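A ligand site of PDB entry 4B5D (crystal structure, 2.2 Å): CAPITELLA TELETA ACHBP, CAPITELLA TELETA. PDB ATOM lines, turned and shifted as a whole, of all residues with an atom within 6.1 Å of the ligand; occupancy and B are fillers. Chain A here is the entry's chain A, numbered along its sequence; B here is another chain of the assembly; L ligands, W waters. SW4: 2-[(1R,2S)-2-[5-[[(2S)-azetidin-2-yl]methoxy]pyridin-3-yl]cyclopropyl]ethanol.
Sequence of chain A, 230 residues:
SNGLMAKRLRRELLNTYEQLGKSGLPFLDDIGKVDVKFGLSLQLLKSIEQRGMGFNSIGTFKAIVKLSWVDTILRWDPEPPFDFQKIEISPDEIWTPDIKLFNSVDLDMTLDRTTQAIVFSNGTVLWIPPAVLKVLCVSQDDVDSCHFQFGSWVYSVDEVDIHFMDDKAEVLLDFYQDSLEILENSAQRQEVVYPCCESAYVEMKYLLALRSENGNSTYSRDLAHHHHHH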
ATOM      1  N   PHE A 102      30.612 -15.439  -8.151  1.00  0.00           N
ATOM      2  CA  PHE A 102      29.346 -16.156  -8.325  1.00  0.00           C
ATOM      3  C   PHE A 102      29.549 -17.653  -8.215  1.00  0.00           C
ATOM      4  O   PHE A 102      28.736 -18.364  -7.613  1.00  0.00           O
ATOM      5  CB  PHE A 102      28.683 -15.843  -9.672  1.00  0.00           C
ATOM      6  CG  PHE A 102      28.047 -14.472  -9.766  1.00  0.00           C
ATOM      7  CD1 PHE A 102      28.392 -13.457  -8.888  1.00  0.00           C
ATOM      8  CD2 PHE A 102      27.081 -14.204 -10.733  1.00  0.00           C
ATOM      9  CE1 PHE A 102      27.792 -12.183  -8.964  1.00  0.00           C
ATOM     10  CE2 PHE A 102      26.485 -12.945 -10.825  1.00  0.00           C
ATOM     11  CZ  PHE A 102      26.850 -11.932  -9.922  1.00  0.00           C
ATOM     12  N   SER A 152      28.345  -7.585  -9.387  1.00  0.00           N
ATOM     13  CA  SER A 152      27.509  -7.025  -8.325  1.00  0.00           C
ATOM     14  C   SER A 152      26.333  -7.961  -8.156  1.00  0.00           C
ATOM     15  O   SER A 152      25.732  -8.362  -9.152  1.00  0.00           O
ATOM     16  CB  SER A 152      26.972  -5.648  -8.724  1.00  0.00           C
ATOM     17  OG  SER A 152      25.984  -5.186  -7.811  1.00  0.00           O
ATOM     18  N   TRP A 153      25.983  -8.311  -6.920  1.00  0.00           N
ATOM     19  CA  TRP A 153      24.868  -9.240  -6.730  1.00  0.00           C
ATOM     20  C   TRP A 153      23.524  -8.570  -7.038  1.00  0.00           C
ATOM     21  O   TRP A 153      22.710  -9.130  -7.761  1.00  0.00           O
ATOM     22  CB  TRP A 153      24.860  -9.840  -5.317  1.00  0.00           C
ATOM     23  CG  TRP A 153      23.936 -11.052  -5.172  1.00  0.00           C
ATOM     24  CD1 TRP A 153      22.810 -11.145  -4.419  1.00  0.00           C
ATOM     25  CD2 TRP A 153      24.111 -12.325  -5.806  1.00  0.00           C
ATOM     26  NE1 TRP A 153      22.260 -12.406  -4.551  1.00  0.00           N
ATOM     27  CE2 TRP A 153      23.048 -13.149  -5.392  1.00  0.00           C
ATOM     28  CE3 TRP A 153      25.066 -12.838  -6.685  1.00  0.00           C
ATOM     29  CZ2 TRP A 153      22.908 -14.456  -5.826  1.00  0.00           C
ATOM     30  CZ3 TRP A 153      24.927 -14.145  -7.118  1.00  0.00           C
ATOM     31  CH2 TRP A 153      23.853 -14.937  -6.682  1.00  0.00           C
ATOM     32  N   VAL A 154      23.286  -7.380  -6.497  1.00  0.00           N
ATOM     33  CA  VAL A 154      21.975  -6.754  -6.607  1.00  0.00           C
ATOM     34  C   VAL A 154      21.853  -5.579  -7.601  1.00  0.00           C
ATOM     35  O   VAL A 154      20.744  -5.242  -7.983  1.00  0.00           O
ATOM     36  CB  VAL A 154      21.396  -6.281  -5.229  1.00  0.00           C
ATOM     37  CG1 VAL A 154      21.307  -7.440  -4.244  1.00  0.00           C
ATOM     38  CG2 VAL A 154      22.197  -5.085  -4.674  1.00  0.00           C
ATOM     39  N   TYR A 155      22.959  -4.959  -8.013  1.00  0.00           N
ATOM     40  CA  TYR A 155      22.867  -3.762  -8.859  1.00  0.00           C
ATOM     41  C   TYR A 155      23.085  -4.067 -10.348  1.00  0.00           C
ATOM     42  O   TYR A 155      24.101  -4.644 -10.725  1.00  0.00           O
ATOM     43  CB  TYR A 155      23.873  -2.703  -8.432  1.00  0.00           C
ATOM     44  CG  TYR A 155      23.755  -2.226  -6.999  1.00  0.00           C
ATOM     45  CD1 TYR A 155      22.750  -1.344  -6.612  1.00  0.00           C
ATOM     46  CD2 TYR A 155      24.682  -2.615  -6.034  1.00  0.00           C
ATOM     47  CE1 TYR A 155      22.646  -0.899  -5.315  1.00  0.00           C
ATOM     48  CE2 TYR A 155      24.599  -2.162  -4.733  1.00  0.00           C
ATOM     49  CZ  TYR A 155      23.573  -1.301  -4.375  1.00  0.00           C
ATOM     50  OH  TYR A 155      23.478  -0.850  -3.080  1.00  0.00           O
ATOM     51  N   TYR A 194      18.647 -11.726 -16.445  1.00  0.00           N
ATOM     52  CA  TYR A 194      18.188 -12.837 -15.628  1.00  0.00           C
ATOM     53  C   TYR A 194      16.656 -12.950 -15.597  1.00  0.00           C
ATOM     54  O   TYR A 194      15.956 -11.965 -15.843  1.00  0.00           O
ATOM     55  CB  TYR A 194      18.747 -12.713 -14.204  1.00  0.00           C
ATOM     56  CG  TYR A 194      20.184 -13.191 -14.067  1.00  0.00           C
ATOM     57  CD1 TYR A 194      20.448 -14.514 -13.775  1.00  0.00           C
ATOM     58  CD2 TYR A 194      21.251 -12.313 -14.238  1.00  0.00           C
ATOM     59  CE1 TYR A 194      21.755 -14.969 -13.635  1.00  0.00           C
ATOM     60  CE2 TYR A 194      22.558 -12.752 -14.105  1.00  0.00           C
ATOM     61  CZ  TYR A 194      22.814 -14.080 -13.811  1.00  0.00           C
ATOM     62  OH  TYR A 194      24.108 -14.559 -13.681  1.00  0.00           O
ATOM     63  N   CYS A 196      14.771 -13.855 -12.838  1.00  0.00           N
ATOM     64  CA  CYS A 196      14.289 -13.311 -11.561  1.00  0.00           C
ATOM     65  C   CYS A 196      14.146 -11.787 -11.613  1.00  0.00           C
ATOM     66  O   CYS A 196      13.433 -11.189 -10.793  1.00  0.00           O
ATOM     67  CB  CYS A 196      15.262 -13.655 -10.427  1.00  0.00           C
ATOM     68  SG  CYS A 196      16.693 -12.515 -10.255  1.00  0.00           S
ATOM     69  N   CYS A 197      14.833 -11.181 -12.575  1.00  0.00           N
ATOM     70  CA  CYS A 197      15.069  -9.744 -12.582  1.00  0.00           C
ATOM     71  C   CYS A 197      14.674  -9.156 -13.942  1.00  0.00           C
ATOM     72  O   CYS A 197      14.175  -9.884 -14.802  1.00  0.00           O
ATOM     73  CB  CYS A 197      16.536  -9.496 -12.245  1.00  0.00           C
ATOM     74  SG  CYS A 197      17.162 -10.648 -10.968  1.00  0.00           S
ATOM     75  N   GLU A 198      14.912  -7.861 -14.139  1.00  0.00           N
ATOM     76  CA  GLU A 198      14.370  -7.163 -15.302  1.00  0.00           C
ATOM     77  C   GLU A 198      15.372  -6.440 -16.212  1.00  0.00           C
ATOM     78  O   GLU A 198      15.121  -6.235 -17.399  1.00  0.00           O
ATOM     79  CB  GLU A 198      13.278  -6.174 -14.843  1.00  0.00           C
ATOM     80  CG  GLU A 198      13.582  -5.492 -13.515  1.00  0.00           C
ATOM     81  CD  GLU A 198      12.396  -4.710 -12.965  1.00  0.00           C
ATOM     82  OE1 GLU A 198      11.413  -4.514 -13.720  1.00  0.00           O
ATOM     83  OE2 GLU A 198      12.441  -4.299 -11.793  1.00  0.00           O
ATOM     84  N   SER A 199      16.513  -6.043 -15.650  1.00  0.00           N
ATOM     85  CA  SER A 199      17.527  -5.337 -16.425  1.00  0.00           C
ATOM     86  C   SER A 199      18.749  -6.224 -16.682  1.00  0.00           C
ATOM     87  O   SER A 199      18.695  -7.448 -16.490  1.00  0.00           O
ATOM     88  CB  SER A 199      17.924  -4.033 -15.711  1.00  0.00           C
ATOM     89  OG  SER A 199      18.839  -3.282 -16.501  1.00  0.00           O
ATOM     90  N   TYR A 201      22.827  -7.243 -15.903  1.00  0.00           N
ATOM     91  CA  TYR A 201      23.846  -7.234 -14.872  1.00  0.00           C
ATOM     92  C   TYR A 201      25.204  -7.491 -15.492  1.00  0.00           C
ATOM     93  O   TYR A 201      25.347  -8.316 -16.396  1.00  0.00           O
ATOM     94  CB  TYR A 201      23.526  -8.274 -13.797  1.00  0.00           C
ATOM     95  CG  TYR A 201      22.297  -7.889 -13.012  1.00  0.00           C
ATOM     96  CD1 TYR A 201      21.023  -8.075 -13.547  1.00  0.00           C
ATOM     97  CD2 TYR A 201      22.411  -7.290 -11.769  1.00  0.00           C
ATOM     98  CE1 TYR A 201      19.897  -7.705 -12.841  1.00  0.00           C
ATOM     99  CE2 TYR A 201      21.273  -6.915 -11.058  1.00  0.00           C
ATOM    100  CZ  TYR A 201      20.031  -7.120 -11.599  1.00  0.00           C
ATOM    101  OH  TYR A 201      18.914  -6.739 -10.883  1.00  0.00           O
ATOM    102  N   GLU A 203      28.817  -8.946 -15.707  1.00  0.00           N
ATOM    103  CA  GLU A 203      29.652  -9.992 -15.144  1.00  0.00           C
ATOM    104  C   GLU A 203      31.026 -10.060 -15.837  1.00  0.00           C
ATOM    105  O   GLU A 203      31.133  -9.903 -17.062  1.00  0.00           O
ATOM    106  CB  GLU A 203      28.930 -11.352 -15.161  1.00  0.00           C
ATOM    107  CG  GLU A 203      27.527 -11.261 -14.527  1.00  0.00           C
ATOM    108  CD  GLU A 203      26.753 -12.569 -14.500  1.00  0.00           C
ATOM    109  OE1 GLU A 203      27.308 -13.621 -14.896  1.00  0.00           O
ATOM    110  OE2 GLU A 203      25.557 -12.527 -14.063  1.00  0.00           O
ATOM    111  N   LYS B  86      12.162   1.038  -5.227  1.00  0.00           N
ATOM    112  CA  LYS B  86      12.729   0.059  -4.317  1.00  0.00           C
ATOM    113  C   LYS B  86      13.985   0.602  -3.647  1.00  0.00           C
ATOM    114  O   LYS B  86      14.530   1.624  -4.045  1.00  0.00           O
ATOM    115  CB  LYS B  86      13.065  -1.233  -5.043  1.00  0.00           C
ATOM    116  CG  LYS B  86      14.098  -1.063  -6.138  1.00  0.00           C
ATOM    117  CD  LYS B  86      14.239  -2.363  -6.941  1.00  0.00           C
ATOM    118  CE  LYS B  86      14.826  -2.108  -8.319  1.00  0.00           C
ATOM    119  NZ  LYS B  86      16.042  -1.241  -8.277  1.00  0.00           N
ATOM    120  N   THR B 115      24.763 -10.486   1.965  1.00  0.00           N
ATOM    121  CA  THR B 115      24.036 -10.258   0.724  1.00  0.00           C
ATOM    122  C   THR B 115      22.853  -9.332   0.985  1.00  0.00           C
ATOM    123  O   THR B 115      22.042  -9.601   1.878  1.00  0.00           O
ATOM    124  CB  THR B 115      23.482 -11.588   0.191  1.00  0.00           C
ATOM    125  OG1 THR B 115      24.586 -12.456  -0.068  1.00  0.00           O
ATOM    126  CG2 THR B 115      22.635 -11.377  -1.048  1.00  0.00           C
ATOM    127  N   GLN B 116      22.749  -8.237   0.231  1.00  0.00           N
ATOM    128  CA  GLN B 116      21.685  -7.274   0.529  1.00  0.00           C
ATOM    129  C   GLN B 116      20.346  -7.813   0.072  1.00  0.00           C
ATOM    130  O   GLN B 116      20.279  -8.654  -0.815  1.00  0.00           O
ATOM    131  CB  GLN B 116      21.939  -5.916  -0.113  1.00  0.00           C
ATOM    132  CG  GLN B 116      23.188  -5.217   0.342  1.00  0.00           C
ATOM    133  CD  GLN B 116      23.433  -3.929  -0.424  1.00  0.00           C
ATOM    134  OE1 GLN B 116      23.102  -2.836   0.055  1.00  0.00           O
ATOM    135  NE2 GLN B 116      23.989  -4.046  -1.643  1.00  0.00           N
ATOM    136  N   ALA B 117      19.272  -7.335   0.715  1.00  0.00           N
ATOM    137  CA  ALA B 117      17.920  -7.623   0.288  1.00  0.00           C
ATOM    138  C   ALA B 117      17.426  -6.371  -0.413  1.00  0.00           C
ATOM    139  O   ALA B 117      17.925  -5.266  -0.185  1.00  0.00           O
ATOM    140  CB  ALA B 117      17.044  -7.956   1.491  1.00  0.00           C
ATOM    141  N   ILE B 118      16.436  -6.540  -1.282  1.00  0.00           N
ATOM    142  CA  ILE B 118      15.804  -5.407  -1.953  1.00  0.00           C
ATOM    143  C   ILE B 118      14.381  -5.270  -1.423  1.00  0.00           C
ATOM    144  O   ILE B 118      13.673  -6.271  -1.307  1.00  0.00           O
ATOM    145  CB  ILE B 118      15.723  -5.656  -3.472  1.00  0.00           C
ATOM    146  CG1 ILE B 118      17.121  -5.603  -4.092  1.00  0.00           C
ATOM    147  CG2 ILE B 118      14.789  -4.673  -4.130  1.00  0.00           C
ATOM    148  CD1 ILE B 118      17.909  -4.365  -3.709  1.00  0.00           C
ATOM    149  N   PHE B 120      10.683  -3.304  -2.083  1.00  0.00           N
ATOM    150  CA  PHE B 120       9.828  -2.469  -2.920  1.00  0.00           C
ATOM    151  C   PHE B 120       8.890  -1.614  -2.057  1.00  0.00           C
ATOM    152  O   PHE B 120       8.582  -1.992  -0.934  1.00  0.00           O
ATOM    153  CB  PHE B 120       8.984  -3.339  -3.858  1.00  0.00           C
ATOM    154  CG  PHE B 120       9.802  -4.189  -4.802  1.00  0.00           C
ATOM    155  CD1 PHE B 120      10.217  -3.697  -6.032  1.00  0.00           C
ATOM    156  CD2 PHE B 120      10.153  -5.488  -4.452  1.00  0.00           C
ATOM    157  CE1 PHE B 120      10.971  -4.479  -6.901  1.00  0.00           C
ATOM    158  CE2 PHE B 120      10.902  -6.276  -5.309  1.00  0.00           C
ATOM    159  CZ  PHE B 120      11.293  -5.768  -6.548  1.00  0.00           C
ATOM    160  N   LEU B 126      12.642  -8.947  -1.380  1.00  0.00           N
ATOM    161  CA  LEU B 126      13.264 -10.013  -2.151  1.00  0.00           C
ATOM    162  C   LEU B 126      14.690 -10.170  -1.669  1.00  0.00           C
ATOM    163  O   LEU B 126      15.478  -9.228  -1.699  1.00  0.00           O
ATOM    164  CB  LEU B 126      13.265  -9.676  -3.644  1.00  0.00           C
ATOM    165  CG  LEU B 126      13.884 -10.729  -4.564  1.00  0.00           C
ATOM    166  CD1 LEU B 126      13.047 -12.010  -4.583  1.00  0.00           C
ATOM    167  CD2 LEU B 126      14.057 -10.201  -5.996  1.00  0.00           C
ATOM    168  N   TRP B 127      15.026 -11.387  -1.250  1.00  0.00           N
ATOM    169  CA  TRP B 127      16.351 -11.671  -0.712  1.00  0.00           C
ATOM    170  C   TRP B 127      16.856 -12.992  -1.271  1.00  0.00           C
ATOM    171  O   TRP B 127      16.250 -14.037  -1.053  1.00  0.00           O
ATOM    172  CB  TRP B 127      16.318 -11.721   0.817  1.00  0.00           C
ATOM    173  CG  TRP B 127      17.674 -11.889   1.446  1.00  0.00           C
ATOM    174  CD1 TRP B 127      18.850 -11.337   1.022  1.00  0.00           C
ATOM    175  CD2 TRP B 127      17.991 -12.672   2.605  1.00  0.00           C
ATOM    176  NE1 TRP B 127      19.880 -11.700   1.863  1.00  0.00           N
ATOM    177  CE2 TRP B 127      19.377 -12.545   2.837  1.00  0.00           C
ATOM    178  CE3 TRP B 127      17.231 -13.477   3.463  1.00  0.00           C
ATOM    179  CZ2 TRP B 127      20.031 -13.184   3.890  1.00  0.00           C
ATOM    180  CZ3 TRP B 127      17.886 -14.102   4.541  1.00  0.00           C
ATOM    181  CH2 TRP B 127      19.265 -13.962   4.734  1.00  0.00           C
ATOM    182  N   ILE B 128      17.991 -12.930  -1.969  1.00  0.00           N
ATOM    183  CA  ILE B 128      18.511 -14.060  -2.723  1.00  0.00           C
ATOM    184  C   ILE B 128      19.962 -14.422  -2.311  1.00  0.00           C
ATOM    185  O   ILE B 128      20.899 -14.276  -3.084  1.00  0.00           O
ATOM    186  CB  ILE B 128      18.427 -13.727  -4.238  1.00  0.00           C
ATOM    187  CG1 ILE B 128      16.993 -13.336  -4.617  1.00  0.00           C
ATOM    188  CG2 ILE B 128      18.784 -14.917  -5.104  1.00  0.00           C
ATOM    189  CD1 ILE B 128      16.834 -13.031  -6.118  1.00  0.00           C
ATOM    190  N   PHE B 175      20.527 -21.127 -12.045  1.00  0.00           N
ATOM    191  CA  PHE B 175      21.920 -20.786 -11.701  1.00  0.00           C
ATOM    192  C   PHE B 175      22.835 -22.014 -11.799  1.00  0.00           C
ATOM    193  O   PHE B 175      23.973 -21.970 -11.318  1.00  0.00           O
ATOM    194  CB  PHE B 175      22.024 -20.283 -10.266  1.00  0.00           C
ATOM    195  CG  PHE B 175      21.436 -18.912 -10.025  1.00  0.00           C
ATOM    196  CD1 PHE B 175      22.206 -17.769 -10.222  1.00  0.00           C
ATOM    197  CD2 PHE B 175      20.129 -18.775  -9.542  1.00  0.00           C
ATOM    198  CE1 PHE B 175      21.682 -16.511  -9.979  1.00  0.00           C
ATOM    199  CE2 PHE B 175      19.596 -17.522  -9.297  1.00  0.00           C
ATOM    200  CZ  PHE B 175      20.375 -16.387  -9.521  1.00  0.00           C
HETATM  201  O01 SW4 L   1      13.822  -6.750 -10.443  1.00  0.00           O
HETATM  202  C02 SW4 L   1      14.258  -5.799  -9.539  1.00  0.00           C
HETATM  203  C03 SW4 L   1      15.024  -6.326  -8.329  1.00  0.00           C
HETATM  204  C04 SW4 L   1      16.433  -6.681  -8.628  1.00  0.00           C
HETATM  205  C05 SW4 L   1      17.441  -6.119  -7.674  1.00  0.00           C
HETATM  206  C06 SW4 L   1      16.981  -7.540  -7.549  1.00  0.00           C
HETATM  207  C07 SW4 L   1      17.909  -8.606  -6.951  1.00  0.00           C
HETATM  208  C08 SW4 L   1      18.035  -8.931  -5.607  1.00  0.00           C
HETATM  209  N09 SW4 L   1      18.903  -9.932  -5.258  1.00  0.00           N
HETATM  210  C10 SW4 L   1      19.644 -10.592  -6.181  1.00  0.00           C
HETATM  211  C11 SW4 L   1      19.515 -10.277  -7.560  1.00  0.00           C
HETATM  212  O12 SW4 L   1      20.227 -10.930  -8.614  1.00  0.00           O
HETATM  213  C13 SW4 L   1      20.592 -10.240  -9.755  1.00  0.00           C
HETATM  214  C14 SW4 L   1      21.570 -10.964 -10.637  1.00  0.00           C
HETATM  215  C15 SW4 L   1      21.562 -12.391 -10.301  1.00  0.00           C
HETATM  216  C16 SW4 L   1      22.747 -12.177  -9.446  1.00  0.00           C
HETATM  217  N17 SW4 L   1      22.908 -10.865 -10.049  1.00  0.00           N
HETATM  218  C18 SW4 L   1      18.647  -9.267  -7.930  1.00  0.00           C
HETATM  219  O   HOH W   1      24.595 -10.759 -12.160  1.00  0.00           O
HETATM  220  O   HOH W   2      19.677 -10.601  -2.678  1.00  0.00           O
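OE2 of Glu 198 is in hydrogen-bond range of O01 of the ligand, 3.1 Å away.
A nitrogen (N17) of the ligand lies within hydrogen-bond range of the backbone carbonyl oxygen of Trp 153, at 2.9 Å.
OG of Ser 152 lies within hydrogen-bond range of N of Tyr 155, at 3.0 Å.
OH of Tyr 194 lies within hydrogen-bond range of OE2 of Glu 203, 2.5 Å away.
The side-chain sulfur (SG) of Cys 196 is disulfide-bonded to the side-chain sulfur (SG) of Cys 197 (2.1 Å).
The backbone carbonyl oxygen of Ile 128 of chain B sits at hydrogen-bond distance from the indole nitrogen of Trp 153, 2.7 Å away.
The backbone NH (N) of Leu 126 of chain B lies within hydrogen-bond range of the backbone carbonyl oxygen (O) of Ile 118 of chain B (2.9 Å).
Merely in contact with the ligand: Ser 152 (3.9 Å), Val 154 (3.4 Å), Tyr 194 (3.9 Å), Cys 197 (3.7 Å), Tyr 201 (3.4 Å), Lys 86 of chain B (3.9 Å), Ile 118 of chain B (3.6 Å) and Ile 128 of chain B (3.7 Å).
Hydrophobic or aromatic side chains within 4 Å of the ligand: Trp 153, Val 154, Tyr 194, Tyr 201, Ile 118 of chain B and Ile 128 of chain B.
The nearest printed residue that does not touch the ligand is Phe 102 (4.1 Å).
Water W1 lies within hydrogen-bond range of a nitrogen (N17) of the ligand (2.7 Å) and the side-chain carboxylate of Glu 203 (2.8 Å).
Water W2 lies within hydrogen-bond range of the backbone carbonyl oxygen (O) of Gln 116 of chain B (2.8 Å), a nitrogen (N09) of the ligand (2.8 Å) and the backbone NH (N) of Ile 128 of chain B (3.0 Å).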
